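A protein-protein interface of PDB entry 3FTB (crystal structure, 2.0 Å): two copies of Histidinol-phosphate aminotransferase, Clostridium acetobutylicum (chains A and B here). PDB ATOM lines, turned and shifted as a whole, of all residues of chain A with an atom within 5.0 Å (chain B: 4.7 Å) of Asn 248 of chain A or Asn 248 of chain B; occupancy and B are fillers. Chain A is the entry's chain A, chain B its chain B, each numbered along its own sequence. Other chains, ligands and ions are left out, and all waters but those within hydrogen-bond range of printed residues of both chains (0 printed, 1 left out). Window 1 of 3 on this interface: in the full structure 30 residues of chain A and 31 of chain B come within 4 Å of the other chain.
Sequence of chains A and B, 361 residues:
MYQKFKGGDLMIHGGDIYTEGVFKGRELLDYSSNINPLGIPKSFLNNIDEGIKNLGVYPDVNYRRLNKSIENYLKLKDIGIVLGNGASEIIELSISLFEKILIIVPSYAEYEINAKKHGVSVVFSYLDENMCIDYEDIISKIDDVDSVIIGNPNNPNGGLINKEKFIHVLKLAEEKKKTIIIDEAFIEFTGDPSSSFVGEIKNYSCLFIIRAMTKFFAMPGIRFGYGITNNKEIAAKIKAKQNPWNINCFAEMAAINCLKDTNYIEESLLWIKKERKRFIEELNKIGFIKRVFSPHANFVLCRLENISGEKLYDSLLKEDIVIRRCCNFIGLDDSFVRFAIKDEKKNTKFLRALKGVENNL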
ATOM      1  N   TYR A  63     -31.972 -32.144   8.611  1.00  0.00           N
ATOM      2  CA  TYR A  63     -32.184 -33.035   9.764  1.00  0.00           C
ATOM      3  C   TYR A  63     -33.324 -34.052   9.594  1.00  0.00           C
ATOM      4  O   TYR A  63     -34.021 -34.379  10.571  1.00  0.00           O
ATOM      5  CB  TYR A  63     -32.401 -32.223  11.056  1.00  0.00           C
ATOM      6  CG  TYR A  63     -31.177 -31.462  11.534  1.00  0.00           C
ATOM      7  CD1 TYR A  63     -30.114 -32.123  12.134  1.00  0.00           C
ATOM      8  CD2 TYR A  63     -31.089 -30.089  11.382  1.00  0.00           C
ATOM      9  CE1 TYR A  63     -28.997 -31.434  12.563  1.00  0.00           C
ATOM     10  CE2 TYR A  63     -29.975 -29.387  11.810  1.00  0.00           C
ATOM     11  CZ  TYR A  63     -28.932 -30.063  12.398  1.00  0.00           C
ATOM     12  OH  TYR A  63     -27.824 -29.361  12.821  1.00  0.00           O
ATOM     13  N   ASN A  85     -31.217 -25.585  20.065  1.00  0.00           N
ATOM     14  CA  ASN A  85     -30.124 -25.777  20.997  1.00  0.00           C
ATOM     15  C   ASN A  85     -30.710 -25.615  22.403  1.00  0.00           C
ATOM     16  O   ASN A  85     -30.539 -24.577  23.044  1.00  0.00           O
ATOM     17  CB  ASN A  85     -29.040 -24.733  20.716  1.00  0.00           C
ATOM     18  CG  ASN A  85     -27.690 -25.101  21.308  1.00  0.00           C
ATOM     19  OD1 ASN A  85     -27.253 -26.253  21.249  1.00  0.00           O
ATOM     20  ND2 ASN A  85     -27.011 -24.105  21.863  1.00  0.00           N
ATOM     21  N   GLY A 221     -26.665 -31.211  29.119  1.00  0.00           N
ATOM     22  CA  GLY A 221     -25.438 -30.765  28.475  1.00  0.00           C
ATOM     23  C   GLY A 221     -25.409 -30.970  26.967  1.00  0.00           C
ATOM     24  O   GLY A 221     -24.473 -30.540  26.275  1.00  0.00           O
ATOM     25  N   ILE A 222     -26.441 -31.629  26.454  1.00  0.00           N
ATOM     26  CA  ILE A 222     -26.506 -31.948  25.033  1.00  0.00           C
ATOM     27  C   ILE A 222     -27.199 -30.811  24.274  1.00  0.00           C
ATOM     28  O   ILE A 222     -26.950 -30.591  23.082  1.00  0.00           O
ATOM     29  CB  ILE A 222     -27.217 -33.307  24.808  1.00  0.00           C
ATOM     30  CG1 ILE A 222     -26.428 -34.175  23.828  1.00  0.00           C
ATOM     31  CG2 ILE A 222     -28.685 -33.119  24.402  1.00  0.00           C
ATOM     32  CD1 ILE A 222     -26.811 -35.627  23.889  1.00  0.00           C
ATOM     33  N   ARG A 223     -28.054 -30.083  24.991  1.00  0.00           N
ATOM     34  CA  ARG A 223     -28.717 -28.889  24.470  1.00  0.00           C
ATOM     35  C   ARG A 223     -29.692 -29.244  23.353  1.00  0.00           C
ATOM     36  O   ARG A 223     -29.397 -29.045  22.174  1.00  0.00           O
ATOM     37  CB  ARG A 223     -27.683 -27.867  23.975  1.00  0.00           C
ATOM     38  CG  ARG A 223     -26.554 -27.586  24.968  1.00  0.00           C
ATOM     39  CD  ARG A 223     -26.830 -26.392  25.877  1.00  0.00           C
ATOM     40  NE  ARG A 223     -28.015 -26.541  26.722  1.00  0.00           N
ATOM     41  CZ  ARG A 223     -29.133 -25.837  26.569  1.00  0.00           C
ATOM     42  NH1 ARG A 223     -29.229 -24.936  25.601  1.00  0.00           N
ATOM     43  NH2 ARG A 223     -30.159 -26.023  27.379  1.00  0.00           N
ATOM     44  N   ASN A 246     -27.829 -25.705  13.708  1.00  0.00           N
ATOM     45  CA  ASN A 246     -27.788 -25.271  15.109  1.00  0.00           C
ATOM     46  C   ASN A 246     -27.744 -26.438  16.104  1.00  0.00           C
ATOM     47  O   ASN A 246     -27.616 -26.237  17.314  1.00  0.00           O
ATOM     48  CB  ASN A 246     -28.978 -24.370  15.437  1.00  0.00           C
ATOM     49  CG  ASN A 246     -30.303 -25.103  15.339  1.00  0.00           C
ATOM     50  OD1 ASN A 246     -30.518 -25.918  14.438  1.00  0.00           O
ATOM     51  ND2 ASN A 246     -31.200 -24.816  16.269  1.00  0.00           N
ATOM     52  N   ILE A 247     -27.862 -27.656  15.589  1.00  0.00           N
ATOM     53  CA  ILE A 247     -27.942 -28.856  16.422  1.00  0.00           C
ATOM     54  C   ILE A 247     -26.683 -29.698  16.278  1.00  0.00           C
ATOM     55  O   ILE A 247     -26.435 -30.261  15.228  1.00  0.00           O
ATOM     56  CB  ILE A 247     -29.170 -29.723  16.024  1.00  0.00           C
ATOM     57  CG1 ILE A 247     -30.450 -28.892  16.052  1.00  0.00           C
ATOM     58  CG2 ILE A 247     -29.306 -30.956  16.907  1.00  0.00           C
ATOM     59  CD1 ILE A 247     -30.647 -28.119  17.332  1.00  0.00           C
ATOM     60  N   ASN A 248     -25.881 -29.780  17.332  1.00  0.00           N
ATOM     61  CA  ASN A 248     -24.665 -30.600  17.302  1.00  0.00           C
ATOM     62  C   ASN A 248     -24.961 -32.089  17.081  1.00  0.00           C
ATOM     63  O   ASN A 248     -26.086 -32.544  17.292  1.00  0.00           O
ATOM     64  CB  ASN A 248     -23.862 -30.416  18.590  1.00  0.00           C
ATOM     65  CG  ASN A 248     -24.439 -31.207  19.756  1.00  0.00           C
ATOM     66  OD1 ASN A 248     -25.148 -30.659  20.598  1.00  0.00           O
ATOM     67  ND2 ASN A 248     -24.130 -32.496  19.811  1.00  0.00           N
ATOM     68  N   CYS A 249     -23.943 -32.849  16.678  1.00  0.00           N
ATOM     69  CA  CYS A 249     -24.134 -34.243  16.275  1.00  0.00           C
ATOM     70  C   CYS A 249     -24.542 -35.216  17.395  1.00  0.00           C
ATOM     71  O   CYS A 249     -25.269 -36.184  17.142  1.00  0.00           O
ATOM     72  CB  CYS A 249     -22.900 -34.767  15.518  1.00  0.00           C
ATOM     73  SG  CYS A 249     -21.378 -35.016  16.484  1.00  0.00           S
ATOM     74  N   PHE A 250     -24.078 -34.978  18.618  1.00  0.00           N
ATOM     75  CA  PHE A 250     -24.444 -35.839  19.747  1.00  0.00           C
ATOM     76  C   PHE A 250     -25.912 -35.634  20.112  1.00  0.00           C
ATOM     77  O   PHE A 250     -26.655 -36.595  20.348  1.00  0.00           O
ATOM     78  CB  PHE A 250     -23.546 -35.565  20.953  1.00  0.00           C
ATOM     79  CG  PHE A 250     -22.109 -35.940  20.730  1.00  0.00           C
ATOM     80  CD1 PHE A 250     -21.709 -37.268  20.783  1.00  0.00           C
ATOM     81  CD2 PHE A 250     -21.153 -34.967  20.464  1.00  0.00           C
ATOM     82  CE1 PHE A 250     -20.382 -37.611  20.575  1.00  0.00           C
ATOM     83  CE2 PHE A 250     -19.829 -35.312  20.254  1.00  0.00           C
ATOM     84  CZ  PHE A 250     -19.446 -36.637  20.307  1.00  0.00           C
ATOM     85  N   ALA A 251     -26.321 -34.369  20.152  1.00  0.00           N
ATOM     86  CA  ALA A 251     -27.715 -34.021  20.360  1.00  0.00           C
ATOM     87  C   ALA A 251     -28.554 -34.793  19.358  1.00  0.00           C
ATOM     88  O   ALA A 251     -29.528 -35.448  19.725  1.00  0.00           O
ATOM     89  CB  ALA A 251     -27.919 -32.522  20.182  1.00  0.00           C
ATOM     90  N   GLU A 252     -28.162 -34.724  18.089  1.00  0.00           N
ATOM     91  CA  GLU A 252     -28.840 -35.466  17.034  1.00  0.00           C
ATOM     92  C   GLU A 252     -28.857 -36.957  17.340  1.00  0.00           C
ATOM     93  O   GLU A 252     -29.892 -37.610  17.196  1.00  0.00           O
ATOM     94  CB  GLU A 252     -28.159 -35.216  15.694  1.00  0.00           C
ATOM     95  CG  GLU A 252     -28.822 -35.873  14.521  1.00  0.00           C
ATOM     96  CD  GLU A 252     -28.076 -35.608  13.229  1.00  0.00           C
ATOM     97  OE1 GLU A 252     -26.831 -35.709  13.231  1.00  0.00           O
ATOM     98  OE2 GLU A 252     -28.732 -35.295  12.214  1.00  0.00           O
ATOM     99  N   ASN B  85     -22.366 -21.345  18.867  1.00  0.00           N
ATOM    100  CA  ASN B  85     -22.811 -22.666  18.459  1.00  0.00           C
ATOM    101  C   ASN B  85     -22.577 -22.766  16.943  1.00  0.00           C
ATOM    102  O   ASN B  85     -23.517 -22.721  16.137  1.00  0.00           O
ATOM    103  CB  ASN B  85     -24.290 -22.847  18.827  1.00  0.00           C
ATOM    104  CG  ASN B  85     -24.762 -24.260  18.653  1.00  0.00           C
ATOM    105  OD1 ASN B  85     -24.095 -25.205  19.086  1.00  0.00           O
ATOM    106  ND2 ASN B  85     -25.923 -24.424  18.014  1.00  0.00           N
ATOM    107  N   GLY B 221     -19.530 -31.317  13.376  1.00  0.00           N
ATOM    108  CA  GLY B 221     -20.683 -31.785  14.126  1.00  0.00           C
ATOM    109  C   GLY B 221     -20.765 -31.292  15.561  1.00  0.00           C
ATOM    110  O   GLY B 221     -21.840 -31.279  16.155  1.00  0.00           O
ATOM    111  N   ILE B 222     -19.643 -30.873  16.133  1.00  0.00           N
ATOM    112  CA  ILE B 222     -19.657 -30.460  17.537  1.00  0.00           C
ATOM    113  C   ILE B 222     -20.187 -29.033  17.726  1.00  0.00           C
ATOM    114  O   ILE B 222     -20.526 -28.631  18.845  1.00  0.00           O
ATOM    115  CB  ILE B 222     -18.277 -30.628  18.204  1.00  0.00           C
ATOM    116  CG1 ILE B 222     -18.425 -31.316  19.554  1.00  0.00           C
ATOM    117  CG2 ILE B 222     -17.559 -29.297  18.319  1.00  0.00           C
ATOM    118  CD1 ILE B 222     -17.243 -32.190  19.898  1.00  0.00           C
ATOM    119  N   ARG B 223     -20.264 -28.287  16.621  1.00  0.00           N
ATOM    120  CA  ARG B 223     -20.866 -26.947  16.586  1.00  0.00           C
ATOM    121  C   ARG B 223     -20.193 -25.948  17.527  1.00  0.00           C
ATOM    122  O   ARG B 223     -20.777 -25.578  18.549  1.00  0.00           O
ATOM    123  CB  ARG B 223     -22.368 -27.018  16.913  1.00  0.00           C
ATOM    124  CG  ARG B 223     -23.160 -28.022  16.089  1.00  0.00           C
ATOM    125  CD  ARG B 223     -23.433 -27.507  14.687  1.00  0.00           C
ATOM    126  NE  ARG B 223     -22.202 -27.266  13.943  1.00  0.00           N
ATOM    127  CZ  ARG B 223     -21.993 -26.223  13.143  1.00  0.00           C
ATOM    128  NH1 ARG B 223     -22.926 -25.290  12.971  1.00  0.00           N
ATOM    129  NH2 ARG B 223     -20.831 -26.103  12.518  1.00  0.00           N
ATOM    130  N   ASN B 246     -25.603 -21.757  25.536  1.00  0.00           N
ATOM    131  CA  ASN B 246     -25.637 -22.107  24.109  1.00  0.00           C
ATOM    132  C   ASN B 246     -24.557 -23.106  23.665  1.00  0.00           C
ATOM    133  O   ASN B 246     -24.674 -23.727  22.601  1.00  0.00           O
ATOM    134  CB  ASN B 246     -25.622 -20.868  23.207  1.00  0.00           C
ATOM    135  CG  ASN B 246     -24.370 -20.043  23.373  1.00  0.00           C
ATOM    136  OD1 ASN B 246     -23.820 -19.943  24.467  1.00  0.00           O
ATOM    137  ND2 ASN B 246     -23.917 -19.436  22.283  1.00  0.00           N
ATOM    138  N   ILE B 247     -23.513 -23.262  24.476  1.00  0.00           N
ATOM    139  CA  ILE B 247     -22.451 -24.207  24.164  1.00  0.00           C
ATOM    140  C   ILE B 247     -22.679 -25.555  24.829  1.00  0.00           C
ATOM    141  O   ILE B 247     -22.827 -25.633  26.044  1.00  0.00           O
ATOM    142  CB  ILE B 247     -21.075 -23.646  24.551  1.00  0.00           C
ATOM    143  CG1 ILE B 247     -20.926 -22.256  23.951  1.00  0.00           C
ATOM    144  CG2 ILE B 247     -19.947 -24.550  24.023  1.00  0.00           C
ATOM    145  CD1 ILE B 247     -20.843 -22.297  22.472  1.00  0.00           C
ATOM    146  N   ASN B 248     -22.721 -26.619  24.032  1.00  0.00           N
ATOM    147  CA  ASN B 248     -22.971 -27.946  24.591  1.00  0.00           C
ATOM    148  C   ASN B 248     -21.710 -28.566  25.187  1.00  0.00           C
ATOM    149  O   ASN B 248     -20.599 -28.237  24.778  1.00  0.00           O
ATOM    150  CB  ASN B 248     -23.646 -28.878  23.567  1.00  0.00           C
ATOM    151  CG  ASN B 248     -22.784 -29.145  22.347  1.00  0.00           C
ATOM    152  OD1 ASN B 248     -22.915 -28.471  21.323  1.00  0.00           O
ATOM    153  ND2 ASN B 248     -21.896 -30.130  22.447  1.00  0.00           N
ATOM    154  N   CYS B 249     -21.893 -29.469  26.149  1.00  0.00           N
ATOM    155  CA  CYS B 249     -20.781 -30.000  26.948  1.00  0.00           C
ATOM    156  C   CYS B 249     -19.646 -30.661  26.140  1.00  0.00           C
ATOM    157  O   CYS B 249     -18.476 -30.594  26.530  1.00  0.00           O
ATOM    158  CB  CYS B 249     -21.297 -30.930  28.067  1.00  0.00           C
ATOM    159  SG  CYS B 249     -22.339 -32.339  27.560  1.00  0.00           S
ATOM    160  N   PHE B 250     -19.978 -31.281  25.018  1.00  0.00           N
ATOM    161  CA  PHE B 250     -18.950 -31.932  24.200  1.00  0.00           C
ATOM    162  C   PHE B 250     -18.058 -30.924  23.487  1.00  0.00           C
ATOM    163  O   PHE B 250     -16.839 -31.094  23.415  1.00  0.00           O
ATOM    164  CB  PHE B 250     -19.579 -32.905  23.201  1.00  0.00           C
ATOM    165  CG  PHE B 250     -20.015 -34.196  23.828  1.00  0.00           C
ATOM    166  CD1 PHE B 250     -19.075 -35.096  24.305  1.00  0.00           C
ATOM    167  CD2 PHE B 250     -21.359 -34.501  23.967  1.00  0.00           C
ATOM    168  CE1 PHE B 250     -19.468 -36.286  24.900  1.00  0.00           C
ATOM    169  CE2 PHE B 250     -21.761 -35.696  24.564  1.00  0.00           C
ATOM    170  CZ  PHE B 250     -20.815 -36.588  25.031  1.00  0.00           C
ATOM    171  N   ALA B 251     -18.689 -29.885  22.951  1.00  0.00           N
ATOM    172  CA  ALA B 251     -17.988 -28.775  22.325  1.00  0.00           C
ATOM    173  C   ALA B 251     -17.119 -28.038  23.337  1.00  0.00           C
ATOM    174  O   ALA B 251     -16.075 -27.490  22.972  1.00  0.00           O
ATOM    175  CB  ALA B 251     -18.995 -27.811  21.676  1.00  0.00           C
ATOM    176  N   GLU B 252     -17.568 -28.027  24.596  1.00  0.00           N
ATOM    177  CA  GLU B 252     -16.835 -27.462  25.736  1.00  0.00           C
ATOM    178  C   GLU B 252     -15.612 -28.308  26.125  1.00  0.00           C
ATOM    179  O   GLU B 252     -14.496 -27.797  26.219  1.00  0.00           O
ATOM    180  CB  GLU B 252     -17.774 -27.290  26.951  1.00  0.00           C
ATOM    181  CG  GLU B 252     -17.139 -26.641  28.166  1.00  0.00           C
ATOM    182  CD  GLU B 252     -17.985 -26.773  29.423  1.00  0.00           C
ATOM    183  OE1 GLU B 252     -18.919 -27.614  29.440  1.00  0.00           O
ATOM    184  OE2 GLU B 252     -17.706 -26.041  30.395  1.00  0.00           O
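O of Asn 246 of chain B lies within hydrogen-bond range of ND2 of Asn 85 of chain A (2.5 Å). O of Gly 221 of chain A sits at hydrogen-bond distance from N of Cys 249 of chain B (2.8 Å). The backbone carbonyl oxygen (O) of Asn 246 of chain A is in hydrogen-bond range of the side-chain amide nitrogen (ND2) of Asn 85 of chain B (2.6 Å). The side-chain amide oxygen (OD1) of Asn 248 of chain B lies close to the side-chain amide oxygen (OD1) of Asn 248 of chain A (3.2 Å). The backbone carbonyl oxygen of Gly 221 of chain B is in hydrogen-bond range of the backbone NH of Cys 249 of chain A.
The side-chain hydroxyl (OH) of Tyr 63 of chain A lies within hydrogen-bond range of the backbone carbonyl oxygen (O) of Ile 247 of chain A (2.9 Å). The backbone carbonyl oxygen (O) of Ile 222 of chain A sits close to the side-chain amide oxygen (OD1) of Asn 248 of chain A, 3.1 Å away. The backbone NH of Ala 251 of chain A sits close to the side-chain amide nitrogen of Asn 248 of chain A (2.9 Å). OD1 of Asn 85 of chain B lies close to O of Arg 223 of chain B, at 3.4 Å. ND2 of Asn 248 of chain B lies close to N of Phe 250 of chain B (3.4 Å). The side-chain amide nitrogen of Asn 248 of chain B lies close to the backbone NH of Ala 251 of chain B, at 3.3 Å.
ND2 of Asn 85 of chain B touches CG of Asn 85 of chain A (3.8 Å). O of Gly 221 of chain A touches CB of Asn 248 of chain B, 3.3 Å away. Ile 222 of chain A touches Asn 248 of chain B (O to CB, 3.8 Å). Asn 248 of chain B touches Arg 223 of chain A (CB to CG, 3.5 Å). C of Ile 247 of chain A touches CG of Arg 223 of chain B, 3.9 Å away. Asn 248 of chain A touches Gly 221 of chain B (CA to O, 3.1 Å). Ile 222 of chain B touches Asn 248 of chain A. Arg 223 of chain B touches Asn 248 of chain A. Phe 250 of chain B touches Phe 250 of chain A.
Of the printed residues of chain B, Gly 221 of chain A touches Asn 248 (3.3 Å) and Cys 249 (2.8 Å). Asn 248 of chain A touches just these residues of chain B: Gly 221 (3.1 Å), Ile 222 (3.8 Å), Arg 223 (3.2 Å) and Asn 248 (3.2 Å). Ile 247 of chain B touches none of the printed residues of chain A. Of the printed residues of chain A, Cys 249 of chain B touches Gly 221. Ala 251 of chain B touches none of the printed residues of chain A. The nearest printed residue of chain B that does not touch Asn 248 of chain A is Asn 85 of chain B (5.2 Å). The nearest residue of chain A that does not touch Asn 248 of chain B is Asn 85 of chain A (4.9 Å). The nearest printed residue of chain A that does not touch Cys 249 of chain B is Ile 222 of chain A (4.3 Å).
Of the 11 printed residues of chain B, 8 touch a printed residue of chain A. Printed residues of chain B that touch a printed residue of chain A: Asn 85, Gly 221, Ile 222, Arg 223, Asn 246, Asn 248, Cys 249 and Phe 250. Hydrophobic or aromatic side chains of chain B within 4 Å of the printed part of chain A: Phe 250. Among the printed residues, no Asp or Glu carboxylate lies within 4 Å of a Lys or Arg side-chain nitrogen of the other chain.
Asn 85 of chain A touches its own counterpart, Asn 85 of chain B. Asn 85 of chain A touches Asn 246 of chain B, and with the chains exchanged Asn 246 of chain A touches Asn 85 of chain B. Gly 221 of chain A touches Asn 248 of chain B, and with the chains exchanged Asn 248 of chain A touches Gly 221 of chain B. Asn 248 of chain A touches its own counterpart, Asn 248 of chain B. 11 positions are printed for both chains.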
